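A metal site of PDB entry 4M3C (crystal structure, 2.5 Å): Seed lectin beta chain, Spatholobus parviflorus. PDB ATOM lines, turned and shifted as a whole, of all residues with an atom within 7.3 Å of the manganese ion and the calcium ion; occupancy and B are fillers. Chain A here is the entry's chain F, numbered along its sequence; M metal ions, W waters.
O of Gly 144 sits at hydrogen-bond distance from N of Glu 126, at 3.0 Å.
A ring nitrogen (ND1) of His 142 lies within hydrogen-bond range of the backbone carbonyl oxygen (O) of Tyr 140 (2.9 Å).
Within 4 Å of the manganese ion: Glu 126, Asp 128, Asp 137 and His 142.
The nearest printed residue that does not touch the manganese ion is Ser 152 (4.2 Å).
The manganese ion is bound by OD2 of Asp 128 (2.1 Å), OE2 of Glu 126 (2.1 Å), water W4 (2.1 Å), NE2 of His 142 (2.2 Å), OD1 of Asp 137 (2.3 Å) and water W3 (2.4 Å).
The manganese ion has six donor atoms within binding distance.
The calcium ion is bound by the side-chain carboxylate (OD2) of Asp 137, water W2, water W1, the side-chain carboxylate (OD2) of Asp 128, the backbone carbonyl oxygen (O) of Tyr 130, the side-chain amide nitrogen (ND2) of Asn 132 and the side-chain carboxylate (OD1) of Asp 128.
The calcium ion has seven donor atoms within binding distance.
Water W3 lies within hydrogen-bond range of the side-chain carboxylate of Glu 126 (2.7 Å) and the backbone carbonyl oxygen of Ile 150 (2.8 Å).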
ATOM      1  N   ASP A  88      23.287  -2.593  17.460  1.00  0.00           N
ATOM      2  CA  ASP A  88      22.548  -3.027  18.644  1.00  0.00           C
ATOM      3  C   ASP A  88      23.356  -2.935  19.932  1.00  0.00           C
ATOM      4  O   ASP A  88      22.779  -2.812  21.006  1.00  0.00           O
ATOM      5  CB  ASP A  88      22.068  -4.476  18.499  1.00  0.00           C
ATOM      6  CG  ASP A  88      20.671  -4.583  17.920  1.00  0.00           C
ATOM      7  OD1 ASP A  88      19.685  -4.539  18.690  1.00  0.00           O
ATOM      8  OD2 ASP A  88      20.584  -4.741  16.693  1.00  0.00           O
ATOM      9  N   GLY A  89      24.687  -3.031  19.820  1.00  0.00           N
ATOM     10  CA  GLY A  89      25.573  -2.864  20.964  1.00  0.00           C
ATOM     11  C   GLY A  89      26.736  -3.855  20.992  1.00  0.00           C
ATOM     12  O   GLY A  89      26.929  -4.644  20.073  1.00  0.00           O
ATOM     13  N   GLY A 105      21.392  -8.920  16.123  1.00  0.00           N
ATOM     14  CA  GLY A 105      20.462  -7.945  16.661  1.00  0.00           C
ATOM     15  C   GLY A 105      20.665  -7.772  18.172  1.00  0.00           C
ATOM     16  O   GLY A 105      21.783  -7.764  18.687  1.00  0.00           O
ATOM     17  N   GLY A 106      19.557  -7.673  18.894  1.00  0.00           N
ATOM     18  CA  GLY A 106      19.581  -7.419  20.320  1.00  0.00           C
ATOM     19  C   GLY A 106      20.092  -8.523  21.227  1.00  0.00           C
ATOM     20  O   GLY A 106      20.249  -8.302  22.424  1.00  0.00           O
ATOM     21  N   PHE A 107      20.359  -9.705  20.686  1.00  0.00           N
ATOM     22  CA  PHE A 107      20.884 -10.791  21.529  1.00  0.00           C
ATOM     23  C   PHE A 107      22.403 -10.708  21.540  1.00  0.00           C
ATOM     24  O   PHE A 107      23.036 -11.393  22.335  1.00  0.00           O
ATOM     25  CB  PHE A 107      20.432 -12.203  21.100  1.00  0.00           C
ATOM     26  CG  PHE A 107      19.037 -12.280  20.522  1.00  0.00           C
ATOM     27  CD1 PHE A 107      17.959 -12.621  21.318  1.00  0.00           C
ATOM     28  CD2 PHE A 107      18.813 -12.059  19.168  1.00  0.00           C
ATOM     29  CE1 PHE A 107      16.681 -12.712  20.768  1.00  0.00           C
ATOM     30  CE2 PHE A 107      17.541 -12.160  18.610  1.00  0.00           C
ATOM     31  CZ  PHE A 107      16.472 -12.481  19.414  1.00  0.00           C
ATOM     32  N   LEU A 108      22.968  -9.876  20.651  1.00  0.00           N
ATOM     33  CA  LEU A 108      24.403  -9.516  20.684  1.00  0.00           C
ATOM     34  C   LEU A 108      25.368 -10.704  20.554  1.00  0.00           C
ATOM     35  O   LEU A 108      26.415 -10.727  21.171  1.00  0.00           O
ATOM     36  CB  LEU A 108      24.739  -8.711  21.976  1.00  0.00           C
ATOM     37  CG  LEU A 108      23.919  -7.524  22.572  1.00  0.00           C
ATOM     38  CD1 LEU A 108      24.618  -6.903  23.801  1.00  0.00           C
ATOM     39  CD2 LEU A 108      23.550  -6.390  21.615  1.00  0.00           C
ATOM     40  N   GLU A 126      27.028  -5.976  28.985  1.00  0.00           N
ATOM     41  CA  GLU A 126      26.640  -5.419  27.696  1.00  0.00           C
ATOM     42  C   GLU A 126      26.634  -3.884  27.739  1.00  0.00           C
ATOM     43  O   GLU A 126      26.429  -3.246  28.809  1.00  0.00           O
ATOM     44  CB  GLU A 126      25.243  -5.923  27.280  1.00  0.00           C
ATOM     45  CG  GLU A 126      24.180  -5.365  28.214  1.00  0.00           C
ATOM     46  CD  GLU A 126      22.751  -5.436  27.730  1.00  0.00           C
ATOM     47  OE1 GLU A 126      22.263  -6.555  27.428  1.00  0.00           O
ATOM     48  OE2 GLU A 126      22.092  -4.376  27.731  1.00  0.00           O
ATOM     49  N   PHE A 127      26.798  -3.310  26.545  1.00  0.00           N
ATOM     50  CA  PHE A 127      26.764  -1.868  26.316  1.00  0.00           C
ATOM     51  C   PHE A 127      25.782  -1.737  25.196  1.00  0.00           C
ATOM     52  O   PHE A 127      26.153  -1.759  24.003  1.00  0.00           O
ATOM     53  CB  PHE A 127      28.161  -1.349  25.932  1.00  0.00           C
ATOM     54  CG  PHE A 127      29.184  -1.552  27.012  1.00  0.00           C
ATOM     55  CD1 PHE A 127      29.423  -0.584  27.954  1.00  0.00           C
ATOM     56  CD2 PHE A 127      29.864  -2.754  27.111  1.00  0.00           C
ATOM     57  CE1 PHE A 127      30.334  -0.783  28.970  1.00  0.00           C
ATOM     58  CE2 PHE A 127      30.780  -2.971  28.154  1.00  0.00           C
ATOM     59  CZ  PHE A 127      31.018  -1.979  29.091  1.00  0.00           C
ATOM     60  N   ASP A 128      24.525  -1.576  25.610  1.00  0.00           N
ATOM     61  CA  ASP A 128      23.377  -1.738  24.738  1.00  0.00           C
ATOM     62  C   ASP A 128      22.844  -0.433  24.087  1.00  0.00           C
ATOM     63  O   ASP A 128      22.338   0.459  24.767  1.00  0.00           O
ATOM     64  CB  ASP A 128      22.297  -2.410  25.572  1.00  0.00           C
ATOM     65  CG  ASP A 128      21.133  -2.890  24.759  1.00  0.00           C
ATOM     66  OD1 ASP A 128      20.845  -2.318  23.692  1.00  0.00           O
ATOM     67  OD2 ASP A 128      20.457  -3.825  25.226  1.00  0.00           O
ATOM     68  N   THR A 129      22.911  -0.326  22.769  1.00  0.00           N
ATOM     69  CA  THR A 129      22.496   0.941  22.166  1.00  0.00           C
ATOM     70  C   THR A 129      21.064   1.050  21.597  1.00  0.00           C
ATOM     71  O   THR A 129      20.724   2.066  20.996  1.00  0.00           O
ATOM     72  CB  THR A 129      23.477   1.427  21.119  1.00  0.00           C
ATOM     73  OG1 THR A 129      23.591   0.427  20.097  1.00  0.00           O
ATOM     74  CG2 THR A 129      24.816   1.738  21.759  1.00  0.00           C
ATOM     75  N   TYR A 130      20.230   0.026  21.808  1.00  0.00           N
ATOM     76  CA  TYR A 130      18.884   0.058  21.238  1.00  0.00           C
ATOM     77  C   TYR A 130      17.891  -0.631  22.158  1.00  0.00           C
ATOM     78  O   TYR A 130      18.171  -1.736  22.626  1.00  0.00           O
ATOM     79  CB  TYR A 130      18.886  -0.641  19.865  1.00  0.00           C
ATOM     80  CG  TYR A 130      17.500  -0.870  19.288  1.00  0.00           C
ATOM     81  CD1 TYR A 130      16.875   0.106  18.489  1.00  0.00           C
ATOM     82  CD2 TYR A 130      16.826  -2.058  19.526  1.00  0.00           C
ATOM     83  CE1 TYR A 130      15.615  -0.117  17.947  1.00  0.00           C
ATOM     84  CE2 TYR A 130      15.554  -2.284  18.991  1.00  0.00           C
ATOM     85  CZ  TYR A 130      14.948  -1.317  18.206  1.00  0.00           C
ATOM     86  OH  TYR A 130      13.680  -1.537  17.678  1.00  0.00           O
ATOM     87  N   GLU A 131      16.741   0.003  22.364  1.00  0.00           N
ATOM     88  CA  GLU A 131      15.754  -0.565  23.246  1.00  0.00           C
ATOM     89  C   GLU A 131      14.926  -1.707  22.644  1.00  0.00           C
ATOM     90  O   GLU A 131      14.179  -1.520  21.675  1.00  0.00           O
ATOM     91  CB  GLU A 131      14.795   0.469  23.774  1.00  0.00           C
ATOM     92  CG  GLU A 131      13.892  -0.161  24.811  1.00  0.00           C
ATOM     93  CD  GLU A 131      12.738   0.705  25.196  1.00  0.00           C
ATOM     94  OE1 GLU A 131      12.366   1.630  24.423  1.00  0.00           O
ATOM     95  OE2 GLU A 131      12.186   0.437  26.289  1.00  0.00           O
ATOM     96  N   ASN A 132      15.082  -2.890  23.237  1.00  0.00           N
ATOM     97  CA  ASN A 132      14.296  -4.053  22.873  1.00  0.00           C
ATOM     98  C   ASN A 132      13.335  -4.287  24.013  1.00  0.00           C
ATOM     99  O   ASN A 132      13.713  -4.737  25.115  1.00  0.00           O
ATOM    100  CB  ASN A 132      15.191  -5.286  22.674  1.00  0.00           C
ATOM    101  CG  ASN A 132      16.123  -5.155  21.468  1.00  0.00           C
ATOM    102  OD1 ASN A 132      15.850  -5.711  20.408  1.00  0.00           O
ATOM    103  ND2 ASN A 132      17.238  -4.430  21.640  1.00  0.00           N
ATOM    104  N   THR A 133      12.073  -3.947  23.754  1.00  0.00           N
ATOM    105  CA  THR A 133      11.052  -4.075  24.775  1.00  0.00           C
ATOM    106  C   THR A 133      10.860  -5.533  25.151  1.00  0.00           C
ATOM    107  O   THR A 133      10.610  -5.851  26.317  1.00  0.00           O
ATOM    108  CB  THR A 133       9.730  -3.442  24.317  1.00  0.00           C
ATOM    109  OG1 THR A 133       9.535  -3.713  22.915  1.00  0.00           O
ATOM    110  CG2 THR A 133       9.759  -1.933  24.534  1.00  0.00           C
ATOM    111  N   PHE A 135      12.993  -7.719  25.588  1.00  0.00           N
ATOM    112  CA  PHE A 135      14.009  -8.050  26.600  1.00  0.00           C
ATOM    113  C   PHE A 135      13.912  -7.175  27.849  1.00  0.00           C
ATOM    114  O   PHE A 135      14.828  -7.134  28.682  1.00  0.00           O
ATOM    115  CB  PHE A 135      15.398  -7.888  26.026  1.00  0.00           C
ATOM    116  CG  PHE A 135      15.614  -8.560  24.712  1.00  0.00           C
ATOM    117  CD1 PHE A 135      14.819  -9.634  24.303  1.00  0.00           C
ATOM    118  CD2 PHE A 135      16.652  -8.155  23.892  1.00  0.00           C
ATOM    119  CE1 PHE A 135      15.054 -10.253  23.075  1.00  0.00           C
ATOM    120  CE2 PHE A 135      16.890  -8.768  22.672  1.00  0.00           C
ATOM    121  CZ  PHE A 135      16.089  -9.808  22.264  1.00  0.00           C
ATOM    122  N   THR A 136      12.795  -6.477  27.970  1.00  0.00           N
ATOM    123  CA  THR A 136      12.609  -5.445  29.012  1.00  0.00           C
ATOM    124  C   THR A 136      13.819  -4.484  29.201  1.00  0.00           C
ATOM    125  O   THR A 136      14.217  -4.200  30.329  1.00  0.00           O
ATOM    126  CB  THR A 136      11.911  -6.029  30.308  1.00  0.00           C
ATOM    127  OG1 THR A 136      12.071  -5.144  31.430  1.00  0.00           O
ATOM    128  CG2 THR A 136      12.364  -7.465  30.675  1.00  0.00           C
ATOM    129  N   ASP A 137      14.361  -3.986  28.081  1.00  0.00           N
ATOM    130  CA  ASP A 137      15.368  -2.894  28.011  1.00  0.00           C
ATOM    131  C   ASP A 137      14.809  -1.574  28.525  1.00  0.00           C
ATOM    132  O   ASP A 137      13.665  -1.240  28.273  1.00  0.00           O
ATOM    133  CB  ASP A 137      15.814  -2.652  26.554  1.00  0.00           C
ATOM    134  CG  ASP A 137      17.022  -3.465  26.140  1.00  0.00           C
ATOM    135  OD1 ASP A 137      17.806  -3.877  27.021  1.00  0.00           O
ATOM    136  OD2 ASP A 137      17.252  -3.679  24.928  1.00  0.00           O
ATOM    137  N   PRO A 138      15.637  -0.765  29.207  1.00  0.00           N
ATOM    138  CA  PRO A 138      15.112   0.548  29.627  1.00  0.00           C
ATOM    139  C   PRO A 138      15.044   1.535  28.448  1.00  0.00           C
ATOM    140  O   PRO A 138      15.696   1.301  27.422  1.00  0.00           O
ATOM    141  CB  PRO A 138      16.123   1.009  30.696  1.00  0.00           C
ATOM    142  CG  PRO A 138      17.362   0.211  30.451  1.00  0.00           C
ATOM    143  CD  PRO A 138      17.034  -1.004  29.639  1.00  0.00           C
ATOM    144  N   TYR A 140      16.553   4.047  27.400  1.00  0.00           N
ATOM    145  CA  TYR A 140      17.770   4.823  27.185  1.00  0.00           C
ATOM    146  C   TYR A 140      18.905   3.863  26.948  1.00  0.00           C
ATOM    147  O   TYR A 140      18.851   2.721  27.419  1.00  0.00           O
ATOM    148  CB  TYR A 140      18.094   5.743  28.369  1.00  0.00           C
ATOM    149  CG  TYR A 140      17.922   5.125  29.718  1.00  0.00           C
ATOM    150  CD1 TYR A 140      18.820   4.178  30.182  1.00  0.00           C
ATOM    151  CD2 TYR A 140      16.858   5.498  30.561  1.00  0.00           C
ATOM    152  CE1 TYR A 140      18.669   3.575  31.424  1.00  0.00           C
ATOM    153  CE2 TYR A 140      16.695   4.915  31.818  1.00  0.00           C
ATOM    154  CZ  TYR A 140      17.601   3.942  32.260  1.00  0.00           C
ATOM    155  OH  TYR A 140      17.510   3.328  33.498  1.00  0.00           O
ATOM    156  N   HIS A 142      22.166   1.839  27.564  1.00  0.00           N
ATOM    157  CA  HIS A 142      22.523   1.396  28.923  1.00  0.00           C
ATOM    158  C   HIS A 142      23.644   0.424  29.011  1.00  0.00           C
ATOM    159  O   HIS A 142      23.941  -0.326  28.066  1.00  0.00           O
ATOM    160  CB  HIS A 142      21.309   0.792  29.618  1.00  0.00           C
ATOM    161  CG  HIS A 142      20.635  -0.262  28.798  1.00  0.00           C
ATOM    162  ND1 HIS A 142      19.729   0.034  27.850  1.00  0.00           N
ATOM    163  CD2 HIS A 142      20.815  -1.650  28.744  1.00  0.00           C
ATOM    164  CE1 HIS A 142      19.344  -1.096  27.229  1.00  0.00           C
ATOM    165  NE2 HIS A 142      20.010  -2.134  27.782  1.00  0.00           N
ATOM    166  N   ILE A 143      24.281   0.446  30.186  1.00  0.00           N
ATOM    167  CA  ILE A 143      25.184  -0.612  30.646  1.00  0.00           C
ATOM    168  C   ILE A 143      24.357  -1.598  31.453  1.00  0.00           C
ATOM    169  O   ILE A 143      23.471  -1.203  32.194  1.00  0.00           O
ATOM    170  CB  ILE A 143      26.288  -0.036  31.544  1.00  0.00           C
ATOM    171  CG1 ILE A 143      27.126   0.953  30.729  1.00  0.00           C
ATOM    172  CG2 ILE A 143      27.181  -1.151  32.073  1.00  0.00           C
ATOM    173  CD1 ILE A 143      28.207   1.641  31.540  1.00  0.00           C
ATOM    174  N   GLY A 144      24.654  -2.883  31.325  1.00  0.00           N
ATOM    175  CA  GLY A 144      23.881  -3.923  31.999  1.00  0.00           C
ATOM    176  C   GLY A 144      24.706  -5.167  32.238  1.00  0.00           C
ATOM    177  O   GLY A 144      25.725  -5.375  31.566  1.00  0.00           O
ATOM    178  N   ASP A 146      24.437  -9.243  32.190  1.00  0.00           N
ATOM    179  CA  ASP A 146      23.674 -10.345  31.635  1.00  0.00           C
ATOM    180  C   ASP A 146      24.177 -11.667  32.272  1.00  0.00           C
ATOM    181  O   ASP A 146      25.390 -11.990  32.216  1.00  0.00           O
ATOM    182  CB  ASP A 146      23.848 -10.361  30.121  1.00  0.00           C
ATOM    183  CG  ASP A 146      23.245  -9.134  29.444  1.00  0.00           C
ATOM    184  OD1 ASP A 146      22.584  -8.296  30.131  1.00  0.00           O
ATOM    185  OD2 ASP A 146      23.425  -9.008  28.197  1.00  0.00           O
ATOM    186  N   ILE A 150      19.493 -12.357  28.105  1.00  0.00           N
ATOM    187  CA  ILE A 150      19.645 -10.972  27.629  1.00  0.00           C
ATOM    188  C   ILE A 150      18.806  -9.973  28.496  1.00  0.00           C
ATOM    189  O   ILE A 150      18.855  -8.770  28.310  1.00  0.00           O
ATOM    190  CB  ILE A 150      19.314 -10.841  26.122  1.00  0.00           C
ATOM    191  CG1 ILE A 150      19.833  -9.526  25.551  1.00  0.00           C
ATOM    192  CG2 ILE A 150      17.825 -10.965  25.881  1.00  0.00           C
ATOM    193  CD1 ILE A 150      21.297  -9.532  25.215  1.00  0.00           C
ATOM    194  N   SER A 151      18.034 -10.467  29.452  1.00  0.00           N
ATOM    195  CA  SER A 151      17.273  -9.555  30.262  1.00  0.00           C
ATOM    196  C   SER A 151      18.136  -9.254  31.483  1.00  0.00           C
ATOM    197  O   SER A 151      18.194 -10.048  32.414  1.00  0.00           O
ATOM    198  CB  SER A 151      15.934 -10.185  30.631  1.00  0.00           C
ATOM    199  OG  SER A 151      15.041  -9.236  31.215  1.00  0.00           O
ATOM    200  N   SER A 152      18.833  -8.125  31.454  1.00  0.00           N
ATOM    201  CA  SER A 152      19.846  -7.843  32.452  1.00  0.00           C
ATOM    202  C   SER A 152      19.317  -7.993  33.868  1.00  0.00           C
ATOM    203  O   SER A 152      18.237  -7.507  34.128  1.00  0.00           O
ATOM    204  CB  SER A 152      20.343  -6.421  32.262  1.00  0.00           C
ATOM    205  OG  SER A 152      20.749  -6.194  30.935  1.00  0.00           O
ATOM    206  N   THR A 155      20.875  -2.717  35.322  1.00  0.00           N
ATOM    207  CA  THR A 155      21.370  -1.736  34.378  1.00  0.00           C
ATOM    208  C   THR A 155      21.534  -0.376  35.070  1.00  0.00           C
ATOM    209  O   THR A 155      21.071  -0.181  36.197  1.00  0.00           O
ATOM    210  CB  THR A 155      20.378  -1.523  33.219  1.00  0.00           C
ATOM    211  OG1 THR A 155      19.201  -0.849  33.697  1.00  0.00           O
ATOM    212  CG2 THR A 155      19.986  -2.859  32.556  1.00  0.00           C
HETATM  213 MN    MN M   1      20.033  -4.283  27.227  1.00  0.00          MN
HETATM  214 CA    CA M   2      18.922  -3.951  23.379  1.00  0.00          CA
HETATM  215  O   HOH W   1      19.355  -6.247  23.899  1.00  0.00           O
HETATM  216  O   HOH W   2      20.269  -3.929  21.498  1.00  0.00           O
HETATM  217  O   HOH W   3      19.663  -6.597  26.661  1.00  0.00           O
HETATM  218  O   HOH W   4      19.489  -4.996  29.154  1.00  0.00           O
